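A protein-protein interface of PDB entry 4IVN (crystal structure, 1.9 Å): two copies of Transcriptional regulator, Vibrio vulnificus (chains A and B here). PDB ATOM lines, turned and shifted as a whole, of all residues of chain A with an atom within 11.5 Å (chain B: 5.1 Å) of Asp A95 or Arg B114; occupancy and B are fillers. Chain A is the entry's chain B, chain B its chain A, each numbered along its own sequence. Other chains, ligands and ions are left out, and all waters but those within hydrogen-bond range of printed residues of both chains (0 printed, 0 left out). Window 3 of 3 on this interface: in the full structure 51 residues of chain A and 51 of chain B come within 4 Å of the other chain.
No position is printed for both chains. Of the 6 pairs that touch across the chains among the printed residues, none has its exchanged pair printed and touching as well.
The backbone NH (N) of Cys A94 lies within hydrogen-bond range of the side-chain carboxylate (OD2) of Asp A92, 3.3 Å away.
CG2 of Ile B112 touches SG of Cys A94 (3.97 Å). CB of Cys A94 touches NH2 of Arg B114, at 3.4 Å. CD2 of Leu B117 touches SG of Cys A94 (3.7 Å). CB of Ala B109 touches CB of Ala A98 (3.9 Å).
Of the 16 printed residues of chain A, 4 touch a printed residue of chain B. Of the 8 printed residues of chain B, 4 touch a printed residue of chain A. Printed residues of chain B that touch a printed residue of chain A: Ala B109, Ile B112, Arg B114 and Leu B117. Hydrophobic or aromatic side chains of chain B that line the printed part of chain A: Ala B109, Ile B112 and Leu B117. Among the printed residues, Asp or Glu carboxylates within 4 Å of a Lys or Arg side-chain nitrogen of the other chain: Asp A92 with Arg B114 and Asp A95 with Arg B114.
NH2 of Arg B114 lies within salt-bridge range of OD2 of Asp A92. NH2 of Arg B114 lies within salt-bridge range of OD1 of Asp A95 (3.3 Å).
Of the printed residues of chain B, Asp A95 touches Arg B114. Arg B114 touches three residues of chain A. Of chain A, only Cys A94 (3.97 Å) comes within 4 Å of Ile B112. Of chain A, only Cys A94 (3.7 Å) comes within 4 Å of Leu B117. Ala B118 touches none of the printed residues of chain A. Printed residues of chain B within 4 Å of Cys A94: Ile B112 (3.97 Å), Arg B114 (3.4 Å) and Leu B117 (3.7 Å). Of the printed residues of chain B, Ala A98 touches Ala B109 (3.9 Å). The nearest residue of chain B that does not touch Asp A95 is Ala B109 (4.5 Å).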
ATOM      1  N   ASP A  92      14.141  13.312 -12.047  1.00  0.00           N
ATOM      2  CA  ASP A  92      14.831  14.593 -11.981  1.00  0.00           C
ATOM      3  C   ASP A  92      15.812  14.896 -13.170  1.00  0.00           C
ATOM      4  O   ASP A  92      16.679  14.084 -13.459  1.00  0.00           O
ATOM      5  CB  ASP A  92      15.632  14.702 -10.679  1.00  0.00           C
ATOM      6  CG  ASP A  92      16.407  16.031 -10.602  1.00  0.00           C
ATOM      7  OD1 ASP A  92      15.744  17.053 -10.389  1.00  0.00           O
ATOM      8  OD2 ASP A  92      17.652  16.093 -10.793  1.00  0.00           O
ATOM      9  N   ILE A  93      15.744  16.103 -13.750  1.00  0.00           N
ATOM     10  CA  ILE A  93      16.550  16.453 -14.927  1.00  0.00           C
ATOM     11  C   ILE A  93      18.033  16.132 -14.866  1.00  0.00           C
ATOM     12  O   ILE A  93      18.509  15.484 -15.780  1.00  0.00           O
ATOM     13  CB  ILE A  93      16.396  17.912 -15.382  1.00  0.00           C
ATOM     14  CG1 ILE A  93      14.963  18.161 -15.831  1.00  0.00           C
ATOM     15  CG2 ILE A  93      17.319  18.187 -16.565  1.00  0.00           C
ATOM     16  CD1 ILE A  93      14.859  19.091 -17.023  1.00  0.00           C
ATOM     17  N   CYS A  94      18.764  16.559 -13.841  1.00  0.00           N
ATOM     18  CA  CYS A  94      20.200  16.267 -13.827  1.00  0.00           C
ATOM     19  C   CYS A  94      20.460  14.788 -13.835  1.00  0.00           C
ATOM     20  O   CYS A  94      21.384  14.308 -14.530  1.00  0.00           O
ATOM     21  CB  CYS A  94      20.901  16.870 -12.645  1.00  0.00           C
ATOM     22  SG  CYS A  94      20.461  18.603 -12.490  1.00  0.00           S
ATOM     23  N   ASP A  95      19.656  14.065 -13.054  1.00  0.00           N
ATOM     24  CA  ASP A  95      19.908  12.637 -12.880  1.00  0.00           C
ATOM     25  C   ASP A  95      19.506  11.838 -14.102  1.00  0.00           C
ATOM     26  O   ASP A  95      20.203  10.890 -14.474  1.00  0.00           O
ATOM     27  CB  ASP A  95      19.200  12.103 -11.643  1.00  0.00           C
ATOM     28  CG  ASP A  95      19.470  12.938 -10.398  1.00  0.00           C
ATOM     29  OD1 ASP A  95      18.459  13.409  -9.845  1.00  0.00           O
ATOM     30  OD2 ASP A  95      20.659  13.122  -9.996  1.00  0.00           O
ATOM     31  N   VAL A  96      18.390  12.209 -14.721  1.00  0.00           N
ATOM     32  CA  VAL A  96      17.907  11.525 -15.954  1.00  0.00           C
ATOM     33  C   VAL A  96      18.899  11.781 -17.108  1.00  0.00           C
ATOM     34  O   VAL A  96      19.288  10.883 -17.892  1.00  0.00           O
ATOM     35  CB  VAL A  96      16.456  11.969 -16.302  1.00  0.00           C
ATOM     36  CG1 VAL A  96      16.036  11.490 -17.675  1.00  0.00           C
ATOM     37  CG2 VAL A  96      15.448  11.396 -15.267  1.00  0.00           C
ATOM     38  N   SER A  97      19.367  13.007 -17.180  1.00  0.00           N
ATOM     39  CA  SER A  97      20.366  13.358 -18.258  1.00  0.00           C
ATOM     40  C   SER A  97      21.621  12.517 -18.053  1.00  0.00           C
ATOM     41  O   SER A  97      22.201  11.966 -19.008  1.00  0.00           O
ATOM     42  CB  SER A  97      20.746  14.800 -18.103  1.00  0.00           C
ATOM     43  OG  SER A  97      19.602  15.618 -18.238  1.00  0.00           O
ATOM     44  N   ALA A  98      22.043  12.409 -16.788  1.00  0.00           N
ATOM     45  CA  ALA A  98      23.269  11.677 -16.482  1.00  0.00           C
ATOM     46  C   ALA A  98      23.101  10.200 -16.697  1.00  0.00           C
ATOM     47  O   ALA A  98      24.037   9.557 -17.183  1.00  0.00           O
ATOM     48  CB  ALA A  98      23.771  11.938 -15.069  1.00  0.00           C
ATOM     49  N   GLN A  99      21.936   9.649 -16.321  1.00  0.00           N
ATOM     50  CA  GLN A  99      21.706   8.193 -16.397  1.00  0.00           C
ATOM     51  C   GLN A  99      21.627   7.755 -17.882  1.00  0.00           C
ATOM     52  O   GLN A  99      22.183   6.744 -18.320  1.00  0.00           O
ATOM     53  CB  GLN A  99      20.395   7.789 -15.657  1.00  0.00           C
ATOM     54  CG  GLN A  99      20.164   6.291 -15.660  1.00  0.00           C
ATOM     55  CD  GLN A  99      21.287   5.532 -15.004  1.00  0.00           C
ATOM     56  OE1 GLN A  99      21.556   5.710 -13.803  1.00  0.00           O
ATOM     57  NE2 GLN A  99      21.924   4.623 -15.770  1.00  0.00           N
ATOM     58  N   SER A 100      20.951   8.565 -18.669  1.00  0.00           N
ATOM     59  CA  SER A 100      20.874   8.328 -20.057  1.00  0.00           C
ATOM     60  C   SER A 100      22.298   8.287 -20.696  1.00  0.00           C
ATOM     61  O   SER A 100      22.562   7.442 -21.549  1.00  0.00           O
ATOM     62  CB  SER A 100      19.919   9.373 -20.645  1.00  0.00           C
ATOM     63  OG  SER A 100      19.689   9.134 -21.986  1.00  0.00           O
ATOM     64  N   ALA A 101      23.234   9.113 -20.228  1.00  0.00           N
ATOM     65  CA  ALA A 101      24.607   9.107 -20.798  1.00  0.00           C
ATOM     66  C   ALA A 101      25.444   7.909 -20.239  1.00  0.00           C
ATOM     67  O   ALA A 101      26.232   7.281 -20.939  1.00  0.00           O
ATOM     68  CB  ALA A 101      25.275  10.439 -20.517  1.00  0.00           C
ATOM     69  N   VAL A 102      25.229   7.566 -18.982  1.00  0.00           N
ATOM     70  CA  VAL A 102      25.856   6.391 -18.437  1.00  0.00           C
ATOM     71  C   VAL A 102      25.400   5.153 -19.225  1.00  0.00           C
ATOM     72  O   VAL A 102      26.228   4.306 -19.597  1.00  0.00           O
ATOM     73  CB  VAL A 102      25.477   6.270 -16.958  1.00  0.00           C
ATOM     74  CG1 VAL A 102      25.716   4.845 -16.449  1.00  0.00           C
ATOM     75  CG2 VAL A 102      26.263   7.328 -16.149  1.00  0.00           C
ATOM     76  N   ASP A 103      24.100   5.054 -19.515  1.00  0.00           N
ATOM     77  CA  ASP A 103      23.573   3.905 -20.273  1.00  0.00           C
ATOM     78  C   ASP A 103      24.198   3.748 -21.644  1.00  0.00           C
ATOM     79  O   ASP A 103      24.588   2.630 -22.063  1.00  0.00           O
ATOM     80  CB  ASP A 103      22.042   3.994 -20.383  1.00  0.00           C
ATOM     81  CG  ASP A 103      21.350   3.762 -19.034  1.00  0.00           C
ATOM     82  OD1 ASP A 103      21.985   3.271 -18.087  1.00  0.00           O
ATOM     83  OD2 ASP A 103      20.153   4.057 -18.919  1.00  0.00           O
ATOM     84  N   SER A 104      24.306   4.868 -22.347  1.00  0.00           N
ATOM     85  CA  SER A 104      24.913   4.874 -23.672  1.00  0.00           C
ATOM     86  C   SER A 104      26.384   4.530 -23.611  1.00  0.00           C
ATOM     87  O   SER A 104      26.855   3.856 -24.508  1.00  0.00           O
ATOM     88  CB  SER A 104      24.790   6.225 -24.371  1.00  0.00           C
ATOM     89  OG  SER A 104      23.430   6.610 -24.399  1.00  0.00           O
ATOM     90  N   ARG A 227      22.791   4.230 -29.428  1.00  0.00           N
ATOM     91  CA  ARG A 227      21.760   5.322 -29.587  1.00  0.00           C
ATOM     92  C   ARG A 227      21.780   6.034 -30.921  1.00  0.00           C
ATOM     93  O   ARG A 227      22.255   7.136 -30.982  1.00  0.00           O
ATOM     94  CB  ARG A 227      21.868   6.440 -28.523  1.00  0.00           C
ATOM     95  CG  ARG A 227      21.955   5.891 -27.149  1.00  0.00           C
ATOM     96  CD  ARG A 227      20.656   5.253 -26.659  1.00  0.00           C
ATOM     97  NE  ARG A 227      20.731   5.473 -25.230  1.00  0.00           N
ATOM     98  CZ  ARG A 227      20.099   6.428 -24.540  1.00  0.00           C
ATOM     99  NH1 ARG A 227      19.156   7.231 -25.096  1.00  0.00           N
ATOM    100  NH2 ARG A 227      20.377   6.499 -23.240  1.00  0.00           N
ATOM    101  N   PHE A 237      22.837  14.184 -26.193  1.00  0.00           N
ATOM    102  CA  PHE A 237      24.090  13.962 -25.508  1.00  0.00           C
ATOM    103  C   PHE A 237      24.326  12.421 -25.390  1.00  0.00           C
ATOM    104  O   PHE A 237      25.447  11.958 -25.550  1.00  0.00           O
ATOM    105  CB  PHE A 237      24.024  14.632 -24.125  1.00  0.00           C
ATOM    106  CG  PHE A 237      25.266  14.417 -23.296  1.00  0.00           C
ATOM    107  CD1 PHE A 237      26.544  14.596 -23.862  1.00  0.00           C
ATOM    108  CD2 PHE A 237      25.168  13.995 -21.939  1.00  0.00           C
ATOM    109  CE1 PHE A 237      27.711  14.375 -23.107  1.00  0.00           C
ATOM    110  CE2 PHE A 237      26.349  13.814 -21.167  1.00  0.00           C
ATOM    111  CZ  PHE A 237      27.612  13.980 -21.760  1.00  0.00           C
ATOM    112  N   ALA A 238      23.267  11.647 -25.187  1.00  0.00           N
ATOM    113  CA  ALA A 238      23.344  10.173 -25.151  1.00  0.00           C
ATOM    114  C   ALA A 238      23.950   9.561 -26.459  1.00  0.00           C
ATOM    115  O   ALA A 238      24.716   8.578 -26.422  1.00  0.00           O
ATOM    116  CB  ALA A 238      21.957   9.624 -24.868  1.00  0.00           C
ATOM    117  N   ALA B 109      27.023  14.679 -11.685  1.00  0.00           N
ATOM    118  CA  ALA B 109      25.621  14.675 -11.238  1.00  0.00           C
ATOM    119  C   ALA B 109      25.453  14.914  -9.758  1.00  0.00           C
ATOM    120  O   ALA B 109      24.593  15.697  -9.423  1.00  0.00           O
ATOM    121  CB  ALA B 109      24.832  13.414 -11.673  1.00  0.00           C
ATOM    122  N   ILE B 112      26.362  18.708  -8.869  1.00  0.00           N
ATOM    123  CA  ILE B 112      25.704  19.861  -9.515  1.00  0.00           C
ATOM    124  C   ILE B 112      24.934  20.694  -8.487  1.00  0.00           C
ATOM    125  O   ILE B 112      24.239  20.188  -7.686  1.00  0.00           O
ATOM    126  CB  ILE B 112      24.839  19.475 -10.761  1.00  0.00           C
ATOM    127  CG1 ILE B 112      25.713  19.554 -12.016  1.00  0.00           C
ATOM    128  CG2 ILE B 112      23.632  20.392 -10.916  1.00  0.00           C
ATOM    129  CD1 ILE B 112      25.329  18.528 -13.063  1.00  0.00           C
ATOM    130  N   ASP B 113      25.193  21.987  -8.476  1.00  0.00           N
ATOM    131  CA  ASP B 113      24.529  22.905  -7.549  1.00  0.00           C
ATOM    132  C   ASP B 113      23.260  23.350  -8.256  1.00  0.00           C
ATOM    133  O   ASP B 113      23.326  24.081  -9.244  1.00  0.00           O
ATOM    134  CB  ASP B 113      25.481  24.084  -7.312  1.00  0.00           C
ATOM    135  CG  ASP B 113      24.786  25.290  -6.701  1.00  0.00           C
ATOM    136  OD1 ASP B 113      23.646  25.204  -6.257  1.00  0.00           O
ATOM    137  OD2 ASP B 113      25.409  26.333  -6.719  1.00  0.00           O
ATOM    138  N   ARG B 114      22.122  22.868  -7.777  1.00  0.00           N
ATOM    139  CA  ARG B 114      20.873  23.040  -8.488  1.00  0.00           C
ATOM    140  C   ARG B 114      20.358  24.485  -8.384  1.00  0.00           C
ATOM    141  O   ARG B 114      19.620  24.926  -9.294  1.00  0.00           O
ATOM    142  CB  ARG B 114      19.808  22.073  -7.952  1.00  0.00           C
ATOM    143  CG  ARG B 114      19.817  20.711  -8.661  1.00  0.00           C
ATOM    144  CD  ARG B 114      20.822  19.736  -8.049  1.00  0.00           C
ATOM    145  NE  ARG B 114      20.795  18.346  -8.586  1.00  0.00           N
ATOM    146  CZ  ARG B 114      19.713  17.643  -8.959  1.00  0.00           C
ATOM    147  NH1 ARG B 114      18.493  18.151  -8.902  1.00  0.00           N
ATOM    148  NH2 ARG B 114      19.844  16.403  -9.420  1.00  0.00           N
ATOM    149  N   LYS B 115      20.739  25.178  -7.284  1.00  0.00           N
ATOM    150  CA  LYS B 115      20.411  26.598  -7.090  1.00  0.00           C
ATOM    151  C   LYS B 115      21.141  27.450  -8.151  1.00  0.00           C
ATOM    152  O   LYS B 115      20.501  28.288  -8.739  1.00  0.00           O
ATOM    153  CB  LYS B 115      20.747  27.146  -5.662  1.00  0.00           C
ATOM    154  CG  LYS B 115      20.017  26.460  -4.494  1.00  0.00           C
ATOM    155  CD  LYS B 115      18.494  26.542  -4.677  1.00  0.00           C
ATOM    156  CE  LYS B 115      17.724  26.732  -3.358  1.00  0.00           C
ATOM    157  NZ  LYS B 115      16.255  26.994  -3.624  1.00  0.00           N
ATOM    158  N   SER B 116      22.450  27.234  -8.406  1.00  0.00           N
ATOM    159  CA  SER B 116      23.108  27.947  -9.500  1.00  0.00           C
ATOM    160  C   SER B 116      22.510  27.651 -10.843  1.00  0.00           C
ATOM    161  O   SER B 116      22.412  28.535 -11.662  1.00  0.00           O
ATOM    162  CB  SER B 116      24.643  27.670  -9.668  1.00  0.00           C
ATOM    163  OG  SER B 116      25.397  27.944  -8.470  1.00  0.00           O
ATOM    164  N   LEU B 117      22.323  26.350 -11.122  1.00  0.00           N
ATOM    165  CA  LEU B 117      21.794  25.861 -12.375  1.00  0.00           C
ATOM    166  C   LEU B 117      20.470  26.609 -12.717  1.00  0.00           C
ATOM    167  O   LEU B 117      20.326  27.097 -13.878  1.00  0.00           O
ATOM    168  CB  LEU B 117      21.543  24.342 -12.270  1.00  0.00           C
ATOM    169  CG  LEU B 117      20.953  23.700 -13.538  1.00  0.00           C
ATOM    170  CD1 LEU B 117      21.829  23.899 -14.788  1.00  0.00           C
ATOM    171  CD2 LEU B 117      20.631  22.218 -13.318  1.00  0.00           C
ATOM    172  N   ALA B 118      19.527  26.671 -11.753  1.00  0.00           N
ATOM    173  CA  ALA B 118      18.217  27.376 -12.015  1.00  0.00           C
ATOM    174  C   ALA B 118      18.436  28.844 -12.383  1.00  0.00           C
ATOM    175  O   ALA B 118      17.846  29.350 -13.351  1.00  0.00           O
ATOM    176  CB  ALA B 118      17.235  27.220 -10.840  1.00  0.00           C
